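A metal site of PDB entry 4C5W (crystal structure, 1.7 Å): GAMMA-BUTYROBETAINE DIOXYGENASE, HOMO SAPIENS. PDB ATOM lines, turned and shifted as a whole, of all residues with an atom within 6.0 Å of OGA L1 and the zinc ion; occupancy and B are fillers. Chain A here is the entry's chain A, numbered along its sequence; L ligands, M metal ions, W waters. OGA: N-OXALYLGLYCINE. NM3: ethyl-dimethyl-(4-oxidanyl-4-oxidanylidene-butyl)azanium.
O4 of OGA L1 lies within salt-bridge range of NH1 of Arg 349, 3.0 Å away. The side-chain amide nitrogen (ND2) of Asn 292 lies within hydrogen-bond range of an oxygen (O4) of NM3 L2 (2.9 Å). The guanidinium group of Arg 360 lies within salt-bridge range of an oxygen (O3) of OGA L1, 2.8 Å away. The side-chain amide nitrogen of Asn 191 is in hydrogen-bond range of an oxygen (O7) of NM3 L2 (2.9 Å).
OD1 of Asn 191 sits at hydrogen-bond distance from N of Ala 193, 3.0 Å away. The guanidinium group (NH2) of Arg 360 is in hydrogen-bond range of the backbone carbonyl oxygen (O) of Gly 227, 2.9 Å away. OD2 of Asp 204 lies close to NE2 of Gln 215 (3.2 Å). N of Val 183 sits at hydrogen-bond distance from O of Leu 362 (2.7 Å). The backbone carbonyl oxygen (O) of Ala 193 is in hydrogen-bond range of the guanidinium group (NH1) of Arg 349 (3.0 Å). The side-chain hydroxyl of Tyr 366 lies within hydrogen-bond range of the side-chain carboxylate of Asp 204 (2.6 Å). N of Leu 199 is in hydrogen-bond range of O of Arg 349, at 2.8 Å.
CG1 of Val 183 touches O4 of OGA L1, at 3.5 Å. CB of Ala 193 touches O1 of OGA L1 (3.2 Å). CD1 of Leu 199 touches C2 of OGA L1, 3.6 Å away. CD1 of Leu 362 touches O3 of OGA L1 (3.5 Å). Hydrophobic or aromatic side chains within 4 Å of OGA L1: Val 183, Ala 193, Leu 199, His 202, His 347 and Leu 362. Within 4 Å of OGA L1: Val 183, Ala 193, Leu 199, His 202, Asp 204, His 347, Arg 349, Arg 360 and Leu 362. The nearest printed residue that does not touch OGA L1 is Leu 217 (4.1 Å).
Within 4 Å of the zinc ion: His 202, Asp 204 and His 347. Along chain A the residues within 4 Å of the zinc ion span positions 202 to 347. The nearest printed residue that does not touch the zinc ion is Gln 215 (4.1 Å).
The zinc ion is bound by an oxygen (O2) of OGA L1 (2.0 Å), the side-chain carboxylate (OD1) of Asp 204 (2.0 Å), a ring nitrogen (NE2) of His 347 (2.1 Å), a ring nitrogen (NE2) of His 202 (2.1 Å) and an oxygen (O2') of OGA L1 (2.3 Å). The zinc ion has five donor atoms within binding distance.
Water W1 lies within hydrogen-bond range of OG of Ser 229, O3 of OGA L1 and O of Gly 348.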
ATOM      1  N   TRP A 181      17.205   2.866  13.635  1.00  0.00           N
ATOM      2  CA  TRP A 181      16.973   1.696  14.445  1.00  0.00           C
ATOM      3  C   TRP A 181      18.225   0.844  14.513  1.00  0.00           C
ATOM      4  O   TRP A 181      19.104   0.934  13.624  1.00  0.00           O
ATOM      5  CB  TRP A 181      15.761   0.885  13.980  1.00  0.00           C
ATOM      6  CG  TRP A 181      15.447   1.016  12.535  1.00  0.00           C
ATOM      7  CD1 TRP A 181      14.539   1.863  11.977  1.00  0.00           C
ATOM      8  CD2 TRP A 181      16.081   0.328  11.452  1.00  0.00           C
ATOM      9  NE1 TRP A 181      14.546   1.736  10.623  1.00  0.00           N
ATOM     10  CE2 TRP A 181      15.479   0.803  10.259  1.00  0.00           C
ATOM     11  CE3 TRP A 181      17.066  -0.671  11.372  1.00  0.00           C
ATOM     12  CZ2 TRP A 181      15.853   0.327   9.007  1.00  0.00           C
ATOM     13  CZ3 TRP A 181      17.423  -1.141  10.146  1.00  0.00           C
ATOM     14  CH2 TRP A 181      16.806  -0.652   8.959  1.00  0.00           C
ATOM     15  N   VAL A 183      20.039  -2.719  14.651  1.00  0.00           N
ATOM     16  CA  VAL A 183      19.994  -4.136  14.339  1.00  0.00           C
ATOM     17  C   VAL A 183      21.030  -4.817  15.220  1.00  0.00           C
ATOM     18  O   VAL A 183      22.220  -4.735  14.978  1.00  0.00           O
ATOM     19  CB  VAL A 183      20.251  -4.432  12.853  1.00  0.00           C
ATOM     20  CG1 VAL A 183      20.060  -5.900  12.588  1.00  0.00           C
ATOM     21  CG2 VAL A 183      19.334  -3.569  11.980  1.00  0.00           C
ATOM     22  N   ASN A 191      11.107  -8.304  16.667  1.00  0.00           N
ATOM     23  CA  ASN A 191      11.275  -8.528  15.239  1.00  0.00           C
ATOM     24  C   ASN A 191      12.384  -9.559  15.042  1.00  0.00           C
ATOM     25  O   ASN A 191      13.366  -9.523  15.759  1.00  0.00           O
ATOM     26  CB  ASN A 191      11.635  -7.192  14.568  1.00  0.00           C
ATOM     27  CG  ASN A 191      11.505  -7.231  13.040  1.00  0.00           C
ATOM     28  OD1 ASN A 191      12.342  -7.796  12.348  1.00  0.00           O
ATOM     29  ND2 ASN A 191      10.452  -6.627  12.523  1.00  0.00           N
ATOM     30  N   ALA A 193      14.591  -9.663  12.886  1.00  0.00           N
ATOM     31  CA  ALA A 193      15.844  -8.953  12.605  1.00  0.00           C
ATOM     32  C   ALA A 193      16.726  -8.742  13.847  1.00  0.00           C
ATOM     33  O   ALA A 193      17.963  -8.764  13.787  1.00  0.00           O
ATOM     34  CB  ALA A 193      15.551  -7.616  11.950  1.00  0.00           C
ATOM     35  N   TYR A 194      16.067  -8.572  14.984  1.00  0.00           N
ATOM     36  CA  TYR A 194      16.753  -8.268  16.234  1.00  0.00           C
ATOM     37  C   TYR A 194      17.091  -9.553  17.029  1.00  0.00           C
ATOM     38  O   TYR A 194      16.961  -9.614  18.242  1.00  0.00           O
ATOM     39  CB  TYR A 194      15.883  -7.343  17.052  1.00  0.00           C
ATOM     40  CG  TYR A 194      15.551  -5.997  16.404  1.00  0.00           C
ATOM     41  CD1 TYR A 194      16.406  -5.399  15.464  1.00  0.00           C
ATOM     42  CD2 TYR A 194      14.420  -5.301  16.790  1.00  0.00           C
ATOM     43  CE1 TYR A 194      16.110  -4.159  14.907  1.00  0.00           C
ATOM     44  CE2 TYR A 194      14.103  -4.066  16.225  1.00  0.00           C
ATOM     45  CZ  TYR A 194      14.966  -3.498  15.296  1.00  0.00           C
ATOM     46  OH  TYR A 194      14.684  -2.283  14.753  1.00  0.00           O
ATOM     47  N   LEU A 199      18.500 -14.368   8.175  1.00  0.00           N
ATOM     48  CA  LEU A 199      17.389 -13.751   7.453  1.00  0.00           C
ATOM     49  C   LEU A 199      17.504 -14.170   6.020  1.00  0.00           C
ATOM     50  O   LEU A 199      18.506 -13.873   5.358  1.00  0.00           O
ATOM     51  CB  LEU A 199      17.458 -12.214   7.580  1.00  0.00           C
ATOM     52  CG  LEU A 199      17.449 -11.652   9.002  1.00  0.00           C
ATOM     53  CD1 LEU A 199      17.495 -10.143   8.957  1.00  0.00           C
ATOM     54  CD2 LEU A 199      16.206 -12.126   9.760  1.00  0.00           C
ATOM     55  N   HIS A 202      14.450 -10.999   1.752  1.00  0.00           N
ATOM     56  CA  HIS A 202      13.222 -10.274   1.963  1.00  0.00           C
ATOM     57  C   HIS A 202      13.395  -8.824   1.541  1.00  0.00           C
ATOM     58  O   HIS A 202      14.522  -8.348   1.395  1.00  0.00           O
ATOM     59  CB  HIS A 202      12.876 -10.286   3.463  1.00  0.00           C
ATOM     60  CG  HIS A 202      13.874  -9.582   4.319  1.00  0.00           C
ATOM     61  ND1 HIS A 202      15.085 -10.141   4.654  1.00  0.00           N
ATOM     62  CD2 HIS A 202      13.828  -8.374   4.944  1.00  0.00           C
ATOM     63  CE1 HIS A 202      15.758  -9.294   5.430  1.00  0.00           C
ATOM     64  NE2 HIS A 202      15.011  -8.219   5.610  1.00  0.00           N
ATOM     65  N   THR A 203      12.254  -8.148   1.383  1.00  0.00           N
ATOM     66  CA  THR A 203      12.165  -6.688   1.356  1.00  0.00           C
ATOM     67  C   THR A 203      11.741  -6.260   2.746  1.00  0.00           C
ATOM     68  O   THR A 203      11.085  -7.052   3.435  1.00  0.00           O
ATOM     69  CB  THR A 203      11.142  -6.188   0.303  1.00  0.00           C
ATOM     70  OG1 THR A 203       9.850  -6.724   0.584  1.00  0.00           O
ATOM     71  CG2 THR A 203      11.530  -6.643  -1.081  1.00  0.00           C
ATOM     72  N   ASP A 204      12.101  -5.052   3.162  1.00  0.00           N
ATOM     73  CA  ASP A 204      11.685  -4.549   4.453  1.00  0.00           C
ATOM     74  C   ASP A 204      10.296  -3.929   4.388  1.00  0.00           C
ATOM     75  O   ASP A 204       9.942  -3.197   3.453  1.00  0.00           O
ATOM     76  CB  ASP A 204      12.657  -3.507   5.006  1.00  0.00           C
ATOM     77  CG  ASP A 204      13.798  -4.109   5.816  1.00  0.00           C
ATOM     78  OD1 ASP A 204      14.224  -5.247   5.539  1.00  0.00           O
ATOM     79  OD2 ASP A 204      14.310  -3.441   6.761  1.00  0.00           O
ATOM     80  N   GLN A 215      16.672   1.914   1.629  1.00  0.00           N
ATOM     81  CA  GLN A 215      17.141   1.515   2.938  1.00  0.00           C
ATOM     82  C   GLN A 215      18.638   1.854   3.096  1.00  0.00           C
ATOM     83  O   GLN A 215      19.427   1.704   2.184  1.00  0.00           O
ATOM     84  CB  GLN A 215      16.915   0.012   3.119  1.00  0.00           C
ATOM     85  CG  GLN A 215      17.398  -0.521   4.465  1.00  0.00           C
ATOM     86  CD  GLN A 215      16.884  -1.905   4.803  1.00  0.00           C
ATOM     87  OE1 GLN A 215      17.444  -2.595   5.671  1.00  0.00           O
ATOM     88  NE2 GLN A 215      15.836  -2.313   4.136  1.00  0.00           N
ATOM     89  N   LEU A 217      21.889   0.967   5.722  1.00  0.00           N
ATOM     90  CA  LEU A 217      22.402   0.119   6.805  1.00  0.00           C
ATOM     91  C   LEU A 217      23.883   0.404   7.006  1.00  0.00           C
ATOM     92  O   LEU A 217      24.680   0.224   6.105  1.00  0.00           O
ATOM     93  CB  LEU A 217      22.243  -1.373   6.486  1.00  0.00           C
ATOM     94  CG  LEU A 217      20.914  -2.110   6.617  1.00  0.00           C
ATOM     95  CD1 LEU A 217      21.078  -3.581   6.199  1.00  0.00           C
ATOM     96  CD2 LEU A 217      20.452  -2.011   8.039  1.00  0.00           C
ATOM     97  N   GLY A 227      27.069 -13.570   9.931  1.00  0.00           N
ATOM     98  CA  GLY A 227      26.546 -12.234   9.682  1.00  0.00           C
ATOM     99  C   GLY A 227      26.875 -11.639   8.344  1.00  0.00           C
ATOM    100  O   GLY A 227      26.738 -10.442   8.157  1.00  0.00           O
ATOM    101  N   ASP A 228      27.271 -12.495   7.390  1.00  0.00           N
ATOM    102  CA  ASP A 228      27.491 -12.043   6.008  1.00  0.00           C
ATOM    103  C   ASP A 228      26.196 -11.516   5.401  1.00  0.00           C
ATOM    104  O   ASP A 228      25.107 -12.011   5.743  1.00  0.00           O
ATOM    105  CB  ASP A 228      28.009 -13.188   5.121  1.00  0.00           C
ATOM    106  CG  ASP A 228      29.225 -13.874   5.684  1.00  0.00           C
ATOM    107  OD1 ASP A 228      29.052 -14.572   6.697  1.00  0.00           O
ATOM    108  OD2 ASP A 228      30.328 -13.711   5.114  1.00  0.00           O
ATOM    109  N   SER A 229      26.311 -10.561   4.484  1.00  0.00           N
ATOM    110  CA  SER A 229      25.156 -10.026   3.771  1.00  0.00           C
ATOM    111  C   SER A 229      24.985 -10.724   2.417  1.00  0.00           C
ATOM    112  O   SER A 229      25.941 -11.203   1.821  1.00  0.00           O
ATOM    113  CB  SER A 229      25.329  -8.539   3.524  1.00  0.00           C
ATOM    114  OG  SER A 229      25.421  -7.854   4.738  1.00  0.00           O
ATOM    115  N   ASN A 292       8.341 -10.372   2.827  1.00  0.00           N
ATOM    116  CA  ASN A 292       9.140 -10.702   3.990  1.00  0.00           C
ATOM    117  C   ASN A 292       8.472 -11.914   4.671  1.00  0.00           C
ATOM    118  O   ASN A 292       7.314 -11.820   5.091  1.00  0.00           O
ATOM    119  CB  ASN A 292       9.262  -9.525   4.946  1.00  0.00           C
ATOM    120  CG  ASN A 292      10.164  -9.804   6.154  1.00  0.00           C
ATOM    121  OD1 ASN A 292      10.548 -10.947   6.431  1.00  0.00           O
ATOM    122  ND2 ASN A 292      10.493  -8.773   6.876  1.00  0.00           N
ATOM    123  N   MET A 332      29.893  -6.843   5.505  1.00  0.00           N
ATOM    124  CA  MET A 332      30.110  -5.465   5.912  1.00  0.00           C
ATOM    125  C   MET A 332      31.156  -5.415   7.011  1.00  0.00           C
ATOM    126  O   MET A 332      31.167  -6.265   7.910  1.00  0.00           O
ATOM    127  CB  MET A 332      28.795  -4.860   6.412  1.00  0.00           C
ATOM    128  CG  MET A 332      27.666  -4.934   5.387  1.00  0.00           C
ATOM    129  SD  MET A 332      26.285  -3.881   5.889  1.00  0.00           S
ATOM    130  CE  MET A 332      27.036  -2.289   5.618  1.00  0.00           C
ATOM    131  N   PHE A 340      20.343   1.033  -0.510  1.00  0.00           N
ATOM    132  CA  PHE A 340      19.781   0.243  -1.603  1.00  0.00           C
ATOM    133  C   PHE A 340      18.291   0.465  -1.796  1.00  0.00           C
ATOM    134  O   PHE A 340      17.588   0.995  -0.904  1.00  0.00           O
ATOM    135  CB  PHE A 340      20.127  -1.256  -1.426  1.00  0.00           C
ATOM    136  CG  PHE A 340      19.644  -1.877  -0.128  1.00  0.00           C
ATOM    137  CD1 PHE A 340      20.449  -1.848   1.015  1.00  0.00           C
ATOM    138  CD2 PHE A 340      18.409  -2.501  -0.048  1.00  0.00           C
ATOM    139  CE1 PHE A 340      20.035  -2.426   2.203  1.00  0.00           C
ATOM    140  CE2 PHE A 340      17.993  -3.106   1.138  1.00  0.00           C
ATOM    141  CZ  PHE A 340      18.793  -3.060   2.259  1.00  0.00           C
ATOM    142  N   HIS A 347      17.191  -8.665   0.305  1.00  0.00           N
ATOM    143  CA  HIS A 347      18.439  -8.762   1.060  1.00  0.00           C
ATOM    144  C   HIS A 347      18.292  -9.766   2.164  1.00  0.00           C
ATOM    145  O   HIS A 347      17.167 -10.122   2.569  1.00  0.00           O
ATOM    146  CB  HIS A 347      18.861  -7.376   1.612  1.00  0.00           C
ATOM    147  CG  HIS A 347      17.882  -6.760   2.577  1.00  0.00           C
ATOM    148  ND1 HIS A 347      16.719  -6.167   2.166  1.00  0.00           N
ATOM    149  CD2 HIS A 347      17.910  -6.657   3.931  1.00  0.00           C
ATOM    150  CE1 HIS A 347      16.067  -5.703   3.223  1.00  0.00           C
ATOM    151  NE2 HIS A 347      16.751  -6.022   4.311  1.00  0.00           N
ATOM    152  N   GLY A 348      19.428 -10.218   2.674  1.00  0.00           N
ATOM    153  CA  GLY A 348      19.409 -11.179   3.756  1.00  0.00           C
ATOM    154  C   GLY A 348      20.717 -11.153   4.513  1.00  0.00           C
ATOM    155  O   GLY A 348      21.645 -10.424   4.172  1.00  0.00           O
ATOM    156  N   ARG A 349      20.789 -12.012   5.511  1.00  0.00           N
ATOM    157  CA  ARG A 349      21.935 -12.104   6.356  1.00  0.00           C
ATOM    158  C   ARG A 349      22.108 -13.559   6.825  1.00  0.00           C
ATOM    159  O   ARG A 349      21.139 -14.238   7.133  1.00  0.00           O
ATOM    160  CB  ARG A 349      21.684 -11.212   7.562  1.00  0.00           C
ATOM    161  CG  ARG A 349      22.364 -11.651   8.821  1.00  0.00           C
ATOM    162  CD  ARG A 349      21.838 -10.883  10.007  1.00  0.00           C
ATOM    163  NE  ARG A 349      20.811 -11.575  10.765  1.00  0.00           N
ATOM    164  CZ  ARG A 349      19.986 -10.957  11.606  1.00  0.00           C
ATOM    165  NH1 ARG A 349      20.030  -9.623  11.771  1.00  0.00           N
ATOM    166  NH2 ARG A 349      19.080 -11.663  12.281  1.00  0.00           N
ATOM    167  N   ARG A 360      27.582  -7.653  17.322  1.00  0.00           N
ATOM    168  CA  ARG A 360      27.189  -7.200  15.993  1.00  0.00           C
ATOM    169  C   ARG A 360      26.104  -6.136  16.137  1.00  0.00           C
ATOM    170  O   ARG A 360      25.144  -6.304  16.891  1.00  0.00           O
ATOM    171  CB  ARG A 360      26.674  -8.360  15.155  1.00  0.00           C
ATOM    172  CG  ARG A 360      26.529  -8.017  13.676  1.00  0.00           C
ATOM    173  CD  ARG A 360      25.952  -9.213  12.951  1.00  0.00           C
ATOM    174  NE  ARG A 360      25.894  -9.066  11.499  1.00  0.00           N
ATOM    175  CZ  ARG A 360      24.873  -8.566  10.802  1.00  0.00           C
ATOM    176  NH1 ARG A 360      23.810  -8.074  11.422  1.00  0.00           N
ATOM    177  NH2 ARG A 360      24.947  -8.522   9.468  1.00  0.00           N
ATOM    178  N   LEU A 362      24.242  -3.024  13.553  1.00  0.00           N
ATOM    179  CA  LEU A 362      24.033  -2.113  12.453  1.00  0.00           C
ATOM    180  C   LEU A 362      23.044  -1.028  12.895  1.00  0.00           C
ATOM    181  O   LEU A 362      22.125  -1.297  13.688  1.00  0.00           O
ATOM    182  CB  LEU A 362      23.492  -2.839  11.223  1.00  0.00           C
ATOM    183  CG  LEU A 362      23.992  -4.226  10.888  1.00  0.00           C
ATOM    184  CD1 LEU A 362      23.230  -4.758   9.686  1.00  0.00           C
ATOM    185  CD2 LEU A 362      25.483  -4.187  10.620  1.00  0.00           C
ATOM    186  N   TYR A 366      15.361   4.496   6.755  1.00  0.00           N
ATOM    187  CA  TYR A 366      14.661   4.422   5.498  1.00  0.00           C
ATOM    188  C   TYR A 366      14.512   5.819   4.905  1.00  0.00           C
ATOM    189  O   TYR A 366      14.498   6.828   5.621  1.00  0.00           O
ATOM    190  CB  TYR A 366      13.268   3.864   5.739  1.00  0.00           C
ATOM    191  CG  TYR A 366      13.222   2.443   6.255  1.00  0.00           C
ATOM    192  CD1 TYR A 366      13.802   1.394   5.539  1.00  0.00           C
ATOM    193  CD2 TYR A 366      12.518   2.149   7.420  1.00  0.00           C
ATOM    194  CE1 TYR A 366      13.727   0.095   6.011  1.00  0.00           C
ATOM    195  CE2 TYR A 366      12.431   0.860   7.867  1.00  0.00           C
ATOM    196  CZ  TYR A 366      13.036  -0.164   7.173  1.00  0.00           C
ATOM    197  OH  TYR A 366      12.910  -1.471   7.679  1.00  0.00           O
HETATM  198  C1  OGA L   1      16.890  -6.168   8.677  1.00  0.00           C
HETATM  199  C2  OGA L   1      18.037  -6.705   7.957  1.00  0.00           C
HETATM  200  C4  OGA L   1      20.362  -7.282   7.733  1.00  0.00           C
HETATM  201  C5  OGA L   1      21.545  -7.604   8.626  1.00  0.00           C
HETATM  202  O1  OGA L   1      17.070  -5.807   9.854  1.00  0.00           O
HETATM  203  O2  OGA L   1      15.780  -6.063   8.063  1.00  0.00           O
HETATM  204  O2' OGA L   1      17.850  -7.063   6.821  1.00  0.00           O
HETATM  205  O3  OGA L   1      22.623  -7.744   8.042  1.00  0.00           O
HETATM  206  N1  OGA L   1      19.240  -6.790   8.513  1.00  0.00           N
HETATM  207  O4  OGA L   1      21.388  -7.726   9.889  1.00  0.00           O
HETATM  208  N1  NM3 L   2      13.399  -3.491  10.976  1.00  0.00           N
HETATM  209  C8  NM3 L   2      12.960  -4.148  12.245  1.00  0.00           C
HETATM  210  O4  NM3 L   2       9.608  -6.107   7.527  1.00  0.00           O
HETATM  211  C5  NM3 L   2      10.342  -5.970   8.534  1.00  0.00           C
HETATM  212  O7  NM3 L   2       9.931  -6.075   9.710  1.00  0.00           O
HETATM  213  C6  NM3 L   2      11.804  -5.754   8.237  1.00  0.00           C
HETATM  214  C2  NM3 L   2      12.530  -3.960   9.856  1.00  0.00           C
HETATM  215  C9  NM3 L   2      13.253  -2.012  11.069  1.00  0.00           C
HETATM  216  C10 NM3 L   2      14.821  -3.788  10.760  1.00  0.00           C
HETATM  217  C3  NM3 L   2      12.670  -5.418   9.463  1.00  0.00           C
HETATM  218 ZN    ZN M   1      15.821  -6.380   6.114  1.00  0.00          ZN
HETATM  219  O   HOH W   1      22.871  -7.878   5.361  1.00  0.00           O
